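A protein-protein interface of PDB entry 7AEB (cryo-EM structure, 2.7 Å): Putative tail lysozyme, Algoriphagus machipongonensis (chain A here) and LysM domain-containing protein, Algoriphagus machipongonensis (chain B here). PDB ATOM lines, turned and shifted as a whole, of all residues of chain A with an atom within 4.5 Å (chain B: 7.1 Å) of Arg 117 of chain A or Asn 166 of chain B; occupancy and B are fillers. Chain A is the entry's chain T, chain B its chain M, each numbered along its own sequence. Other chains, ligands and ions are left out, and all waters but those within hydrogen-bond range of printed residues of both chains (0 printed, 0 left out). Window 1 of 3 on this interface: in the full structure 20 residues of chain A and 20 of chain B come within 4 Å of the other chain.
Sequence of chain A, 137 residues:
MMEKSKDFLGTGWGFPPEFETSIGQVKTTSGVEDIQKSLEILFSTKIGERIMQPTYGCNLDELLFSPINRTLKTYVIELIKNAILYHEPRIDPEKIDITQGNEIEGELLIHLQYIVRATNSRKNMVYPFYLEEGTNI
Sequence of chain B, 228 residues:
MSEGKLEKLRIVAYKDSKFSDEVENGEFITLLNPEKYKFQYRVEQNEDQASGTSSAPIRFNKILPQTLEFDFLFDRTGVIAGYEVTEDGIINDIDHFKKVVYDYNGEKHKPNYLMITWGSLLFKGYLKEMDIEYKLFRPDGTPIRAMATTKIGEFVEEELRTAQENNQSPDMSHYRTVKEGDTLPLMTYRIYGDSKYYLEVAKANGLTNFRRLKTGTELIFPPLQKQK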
ATOM      1  N   PHE A   8      -7.167 -19.117 -36.318  1.00  0.00           N
ATOM      2  CA  PHE A   8      -7.353 -19.354 -34.886  1.00  0.00           C
ATOM      3  C   PHE A   8      -8.137 -18.253 -34.204  1.00  0.00           C
ATOM      4  O   PHE A   8      -8.322 -18.303 -32.984  1.00  0.00           O
ATOM      5  CB  PHE A   8      -6.024 -19.616 -34.127  1.00  0.00           C
ATOM      6  CG  PHE A   8      -5.003 -18.518 -34.156  1.00  0.00           C
ATOM      7  CD1 PHE A   8      -5.076 -17.422 -33.308  1.00  0.00           C
ATOM      8  CD2 PHE A   8      -3.891 -18.656 -34.951  1.00  0.00           C
ATOM      9  CE1 PHE A   8      -4.110 -16.467 -33.320  1.00  0.00           C
ATOM     10  CE2 PHE A   8      -2.919 -17.700 -34.954  1.00  0.00           C
ATOM     11  CZ  PHE A   8      -3.030 -16.606 -34.140  1.00  0.00           C
ATOM     12  N   PRO A  89      -9.613 -13.708 -24.606  1.00  0.00           N
ATOM     13  CA  PRO A  89      -8.219 -14.163 -24.839  1.00  0.00           C
ATOM     14  C   PRO A  89      -7.521 -13.647 -26.085  1.00  0.00           C
ATOM     15  O   PRO A  89      -6.302 -13.821 -26.215  1.00  0.00           O
ATOM     16  CB  PRO A  89      -8.400 -15.682 -24.972  1.00  0.00           C
ATOM     17  CG  PRO A  89      -9.679 -15.977 -24.307  1.00  0.00           C
ATOM     18  CD  PRO A  89     -10.549 -14.829 -24.560  1.00  0.00           C
ATOM     19  N   ARG A  90      -8.249 -13.107 -27.042  1.00  0.00           N
ATOM     20  CA  ARG A  90      -7.631 -12.723 -28.297  1.00  0.00           C
ATOM     21  C   ARG A  90      -7.040 -11.314 -28.315  1.00  0.00           C
ATOM     22  O   ARG A  90      -6.409 -10.961 -29.313  1.00  0.00           O
ATOM     23  CB  ARG A  90      -8.650 -12.902 -29.428  1.00  0.00           C
ATOM     24  CG  ARG A  90      -9.020 -14.388 -29.646  1.00  0.00           C
ATOM     25  CD  ARG A  90     -10.177 -14.623 -30.600  1.00  0.00           C
ATOM     26  NE  ARG A  90     -11.425 -14.090 -30.060  1.00  0.00           N
ATOM     27  CZ  ARG A  90     -12.624 -14.134 -30.644  1.00  0.00           C
ATOM     28  NH1 ARG A  90     -12.822 -14.705 -31.819  1.00  0.00           N
ATOM     29  NH2 ARG A  90     -13.652 -13.579 -30.032  1.00  0.00           N
ATOM     30  N   ILE A  91      -7.213 -10.473 -27.279  1.00  0.00           N
ATOM     31  CA  ILE A  91      -6.692  -9.105 -27.362  1.00  0.00           C
ATOM     32  C   ILE A  91      -5.871  -8.667 -26.155  1.00  0.00           C
ATOM     33  O   ILE A  91      -5.994  -9.194 -25.050  1.00  0.00           O
ATOM     34  CB  ILE A  91      -7.798  -8.051 -27.572  1.00  0.00           C
ATOM     35  CG1 ILE A  91      -8.701  -7.951 -26.338  1.00  0.00           C
ATOM     36  CG2 ILE A  91      -8.584  -8.358 -28.813  1.00  0.00           C
ATOM     37  CD1 ILE A  91      -9.639  -6.774 -26.333  1.00  0.00           C
ATOM     38  N   ASP A  92      -5.080  -7.612 -26.384  1.00  0.00           N
ATOM     39  CA  ASP A  92      -4.327  -6.859 -25.372  1.00  0.00           C
ATOM     40  C   ASP A  92      -4.767  -5.400 -25.383  1.00  0.00           C
ATOM     41  O   ASP A  92      -4.589  -4.722 -26.406  1.00  0.00           O
ATOM     42  CB  ASP A  92      -2.823  -6.906 -25.644  1.00  0.00           C
ATOM     43  CG  ASP A  92      -2.168  -8.206 -25.276  1.00  0.00           C
ATOM     44  OD1 ASP A  92      -2.209  -8.606 -24.112  1.00  0.00           O
ATOM     45  OD2 ASP A  92      -1.600  -8.845 -26.173  1.00  0.00           O
ATOM     46  N   ILE A 115      -5.227  -3.956 -29.152  1.00  0.00           N
ATOM     47  CA  ILE A 115      -4.412  -4.627 -30.164  1.00  0.00           C
ATOM     48  C   ILE A 115      -4.778  -6.113 -30.274  1.00  0.00           C
ATOM     49  O   ILE A 115      -4.847  -6.822 -29.265  1.00  0.00           O
ATOM     50  CB  ILE A 115      -2.922  -4.452 -29.833  1.00  0.00           C
ATOM     51  CG1 ILE A 115      -2.582  -2.961 -29.875  1.00  0.00           C
ATOM     52  CG2 ILE A 115      -2.043  -5.263 -30.777  1.00  0.00           C
ATOM     53  CD1 ILE A 115      -1.263  -2.589 -29.279  1.00  0.00           C
ATOM     54  N   VAL A 116      -4.970  -6.591 -31.501  1.00  0.00           N
ATOM     55  CA  VAL A 116      -5.288  -7.999 -31.744  1.00  0.00           C
ATOM     56  C   VAL A 116      -4.007  -8.835 -31.762  1.00  0.00           C
ATOM     57  O   VAL A 116      -3.042  -8.490 -32.448  1.00  0.00           O
ATOM     58  CB  VAL A 116      -6.086  -8.131 -33.052  1.00  0.00           C
ATOM     59  CG1 VAL A 116      -6.340  -9.577 -33.395  1.00  0.00           C
ATOM     60  CG2 VAL A 116      -7.404  -7.392 -32.909  1.00  0.00           C
ATOM     61  N   ARG A 117      -3.997  -9.939 -31.010  1.00  0.00           N
ATOM     62  CA  ARG A 117      -2.825 -10.807 -30.866  1.00  0.00           C
ATOM     63  C   ARG A 117      -2.475 -11.615 -32.123  1.00  0.00           C
ATOM     64  O   ARG A 117      -3.338 -12.230 -32.753  1.00  0.00           O
ATOM     65  CB  ARG A 117      -3.056 -11.779 -29.712  1.00  0.00           C
ATOM     66  CG  ARG A 117      -2.995 -11.119 -28.365  1.00  0.00           C
ATOM     67  CD  ARG A 117      -3.360 -12.049 -27.263  1.00  0.00           C
ATOM     68  NE  ARG A 117      -3.072 -11.420 -25.987  1.00  0.00           N
ATOM     69  CZ  ARG A 117      -3.501 -11.831 -24.797  1.00  0.00           C
ATOM     70  NH1 ARG A 117      -4.287 -12.887 -24.659  1.00  0.00           N
ATOM     71  NH2 ARG A 117      -3.127 -11.163 -23.724  1.00  0.00           N
ATOM     72  N   ALA A 118      -1.177 -11.678 -32.439  1.00  0.00           N
ATOM     73  CA  ALA A 118      -0.659 -12.438 -33.577  1.00  0.00           C
ATOM     74  C   ALA A 118      -0.352 -13.901 -33.264  1.00  0.00           C
ATOM     75  O   ALA A 118       0.022 -14.648 -34.171  1.00  0.00           O
ATOM     76  CB  ALA A 118       0.618 -11.789 -34.098  1.00  0.00           C
ATOM     77  N   THR A 119      -0.397 -14.303 -32.000  1.00  0.00           N
ATOM     78  CA  THR A 119      -0.087 -15.657 -31.546  1.00  0.00           C
ATOM     79  C   THR A 119      -1.292 -16.187 -30.782  1.00  0.00           C
ATOM     80  O   THR A 119      -2.031 -15.396 -30.233  1.00  0.00           O
ATOM     81  CB  THR A 119       1.161 -15.638 -30.643  1.00  0.00           C
ATOM     82  OG1 THR A 119       2.264 -15.091 -31.362  1.00  0.00           O
ATOM     83  CG2 THR A 119       1.556 -17.003 -30.148  1.00  0.00           C
ATOM     84  N   SER A 121      -3.555 -17.748 -27.900  1.00  0.00           N
ATOM     85  CA  SER A 121      -3.675 -17.863 -26.451  1.00  0.00           C
ATOM     86  C   SER A 121      -4.119 -19.244 -25.989  1.00  0.00           C
ATOM     87  O   SER A 121      -4.922 -19.913 -26.637  1.00  0.00           O
ATOM     88  CB  SER A 121      -4.696 -16.865 -25.930  1.00  0.00           C
ATOM     89  OG  SER A 121      -4.948 -17.136 -24.573  1.00  0.00           O
ATOM     90  N   ARG B 161      -3.238 -15.129 -12.569  1.00  0.00           N
ATOM     91  CA  ARG B 161      -1.790 -15.105 -12.764  1.00  0.00           C
ATOM     92  C   ARG B 161      -1.405 -15.634 -14.140  1.00  0.00           C
ATOM     93  O   ARG B 161      -0.542 -15.062 -14.814  1.00  0.00           O
ATOM     94  CB  ARG B 161      -1.090 -15.912 -11.669  1.00  0.00           C
ATOM     95  CG  ARG B 161       0.429 -15.916 -11.821  1.00  0.00           C
ATOM     96  CD  ARG B 161       1.137 -16.793 -10.829  1.00  0.00           C
ATOM     97  NE  ARG B 161       0.665 -18.171 -10.841  1.00  0.00           N
ATOM     98  CZ  ARG B 161       1.128 -19.117 -11.648  1.00  0.00           C
ATOM     99  NH1 ARG B 161       2.068 -18.836 -12.535  1.00  0.00           N
ATOM    100  NH2 ARG B 161       0.640 -20.345 -11.578  1.00  0.00           N
ATOM    101  N   THR B 162      -2.047 -16.714 -14.579  1.00  0.00           N
ATOM    102  CA  THR B 162      -1.789 -17.255 -15.905  1.00  0.00           C
ATOM    103  C   THR B 162      -2.331 -16.372 -17.023  1.00  0.00           C
ATOM    104  O   THR B 162      -1.819 -16.441 -18.141  1.00  0.00           O
ATOM    105  CB  THR B 162      -2.379 -18.661 -16.031  1.00  0.00           C
ATOM    106  OG1 THR B 162      -3.772 -18.631 -15.708  1.00  0.00           O
ATOM    107  CG2 THR B 162      -1.676 -19.622 -15.099  1.00  0.00           C
ATOM    108  N   ALA B 163      -3.340 -15.545 -16.757  1.00  0.00           N
ATOM    109  CA  ALA B 163      -3.816 -14.622 -17.778  1.00  0.00           C
ATOM    110  C   ALA B 163      -2.917 -13.398 -17.896  1.00  0.00           C
ATOM    111  O   ALA B 163      -2.847 -12.782 -18.964  1.00  0.00           O
ATOM    112  CB  ALA B 163      -5.251 -14.202 -17.471  1.00  0.00           C
ATOM    113  N   GLN B 164      -2.228 -13.029 -16.816  1.00  0.00           N
ATOM    114  CA  GLN B 164      -1.291 -11.913 -16.869  1.00  0.00           C
ATOM    115  C   GLN B 164       0.061 -12.351 -17.416  1.00  0.00           C
ATOM    116  O   GLN B 164       0.732 -11.579 -18.106  1.00  0.00           O
ATOM    117  CB  GLN B 164      -1.135 -11.293 -15.481  1.00  0.00           C
ATOM    118  CG  GLN B 164      -2.317 -10.458 -15.045  1.00  0.00           C
ATOM    119  CD  GLN B 164      -2.290 -10.112 -13.572  1.00  0.00           C
ATOM    120  OE1 GLN B 164      -1.968 -10.944 -12.730  1.00  0.00           O
ATOM    121  NE2 GLN B 164      -2.632  -8.875 -13.254  1.00  0.00           N
ATOM    122  N   GLU B 165       0.478 -13.576 -17.105  1.00  0.00           N
ATOM    123  CA  GLU B 165       1.635 -14.208 -17.736  1.00  0.00           C
ATOM    124  C   GLU B 165       1.141 -14.952 -18.969  1.00  0.00           C
ATOM    125  O   GLU B 165       0.932 -16.168 -18.959  1.00  0.00           O
ATOM    126  CB  GLU B 165       2.323 -15.168 -16.779  1.00  0.00           C
ATOM    127  CG  GLU B 165       2.866 -14.547 -15.529  1.00  0.00           C
ATOM    128  CD  GLU B 165       3.324 -15.583 -14.528  1.00  0.00           C
ATOM    129  OE1 GLU B 165       3.216 -16.791 -14.818  1.00  0.00           O
ATOM    130  OE2 GLU B 165       3.797 -15.186 -13.443  1.00  0.00           O
ATOM    131  N   ASN B 166       0.945 -14.208 -20.052  1.00  0.00           N
ATOM    132  CA  ASN B 166       0.452 -14.794 -21.297  1.00  0.00           C
ATOM    133  C   ASN B 166       1.608 -15.572 -21.930  1.00  0.00           C
ATOM    134  O   ASN B 166       2.317 -15.104 -22.823  1.00  0.00           O
ATOM    135  CB  ASN B 166      -0.103 -13.700 -22.205  1.00  0.00           C
ATOM    136  CG  ASN B 166      -0.544 -14.213 -23.549  1.00  0.00           C
ATOM    137  OD1 ASN B 166      -1.102 -15.299 -23.669  1.00  0.00           O
ATOM    138  ND2 ASN B 166      -0.279 -13.431 -24.581  1.00  0.00           N
ATOM    139  N   ASN B 167       1.808 -16.787 -21.427  1.00  0.00           N
ATOM    140  CA  ASN B 167       2.976 -17.591 -21.764  1.00  0.00           C
ATOM    141  C   ASN B 167       2.811 -18.189 -23.152  1.00  0.00           C
ATOM    142  O   ASN B 167       1.855 -18.927 -23.412  1.00  0.00           O
ATOM    143  CB  ASN B 167       3.177 -18.689 -20.725  1.00  0.00           C
ATOM    144  CG  ASN B 167       3.931 -18.205 -19.515  1.00  0.00           C
ATOM    145  OD1 ASN B 167       4.877 -17.435 -19.631  1.00  0.00           O
ATOM    146  ND2 ASN B 167       3.508 -18.640 -18.344  1.00  0.00           N
ATOM    147  N   GLN B 168       3.733 -17.872 -24.048  1.00  0.00           N
ATOM    148  CA  GLN B 168       3.661 -18.384 -25.405  1.00  0.00           C
ATOM    149  C   GLN B 168       4.927 -19.137 -25.786  1.00  0.00           C
ATOM    150  O   GLN B 168       5.028 -20.347 -25.576  1.00  0.00           O
ATOM    151  CB  GLN B 168       3.407 -17.243 -26.383  1.00  0.00           C
ATOM    152  CG  GLN B 168       4.636 -16.469 -26.775  1.00  0.00           C
ATOM    153  CD  GLN B 168       4.304 -15.067 -27.216  1.00  0.00           C
ATOM    154  OE1 GLN B 168       3.456 -14.404 -26.621  1.00  0.00           O
ATOM    155  NE2 GLN B 168       4.970 -14.603 -28.264  1.00  0.00           N
ATOM    156  N   TYR B 175       1.388 -16.315 -37.255  1.00  0.00           N
ATOM    157  CA  TYR B 175       1.310 -15.906 -38.653  1.00  0.00           C
ATOM    158  C   TYR B 175       2.042 -14.583 -38.856  1.00  0.00           C
ATOM    159  O   TYR B 175       2.062 -13.726 -37.972  1.00  0.00           O
ATOM    160  CB  TYR B 175      -0.159 -15.811 -39.158  1.00  0.00           C
ATOM    161  CG  TYR B 175      -1.073 -14.839 -38.434  1.00  0.00           C
ATOM    162  CD1 TYR B 175      -1.123 -13.495 -38.794  1.00  0.00           C
ATOM    163  CD2 TYR B 175      -1.915 -15.270 -37.424  1.00  0.00           C
ATOM    164  CE1 TYR B 175      -1.947 -12.612 -38.143  1.00  0.00           C
ATOM    165  CE2 TYR B 175      -2.751 -14.389 -36.767  1.00  0.00           C
ATOM    166  CZ  TYR B 175      -2.760 -13.063 -37.130  1.00  0.00           C
ATOM    167  OH  TYR B 175      -3.589 -12.180 -36.485  1.00  0.00           O
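O of Arg 90 of chain A lies within hydrogen-bond range of N of Arg 117 of chain A (3.1 Å).
The side-chain carboxylate of Asp 92 of chain A is in salt-bridge range of the guanidinium group of Arg 117 of chain A (2.7 Å).
O of Pro 89 of chain A is in hydrogen-bond range of NH1 of Arg 117 of chain A.
Tyr 175 of chain B touches Phe 8 of chain A.
Asn 166 of chain B touches Arg 117 of chain A (ND2 to CZ, 3.6 Å).
Arg 117 of chain A touches Tyr 175 of chain B (O to OH, 3.7 Å).
Ala 118 of chain A touches Tyr 175 of chain B (O to N, 3.8 Å).
Of the printed residues of chain B, Phe 8 of chain A touches Tyr 175 (3.4 Å).
Ile 91 of chain A touches none of the printed residues of chain B.
Arg 117 of chain A touches two residues of chain B.
Printed residues of chain B within 4 Å of Ala 118 of chain A: Tyr 175 (3.8 Å).
Printed residues of chain A within 4 Å of Tyr 175 of chain B: Phe 8, Arg 117 and Ala 118.
The nearest residue of chain B that does not touch Arg 117 of chain A is Ala 163 of chain B (5.0 Å).
The nearest printed residue of chain B that does not touch Ala 118 of chain A is Gln 168 of chain B (7.3 Å).
Printed residues of chain A that touch a printed residue of chain B: Phe 8, Arg 117 and Ala 118.
Hydrophobic or aromatic side chains of chain A that line the printed part of chain B: Phe 8.
Of the 9 printed residues of chain B, 2 touch a printed residue of chain A.
Hydrophobic or aromatic side chains of chain B that line the printed part of chain A: Tyr 175.
Among the printed residues, 4 pairs touch across the chains.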
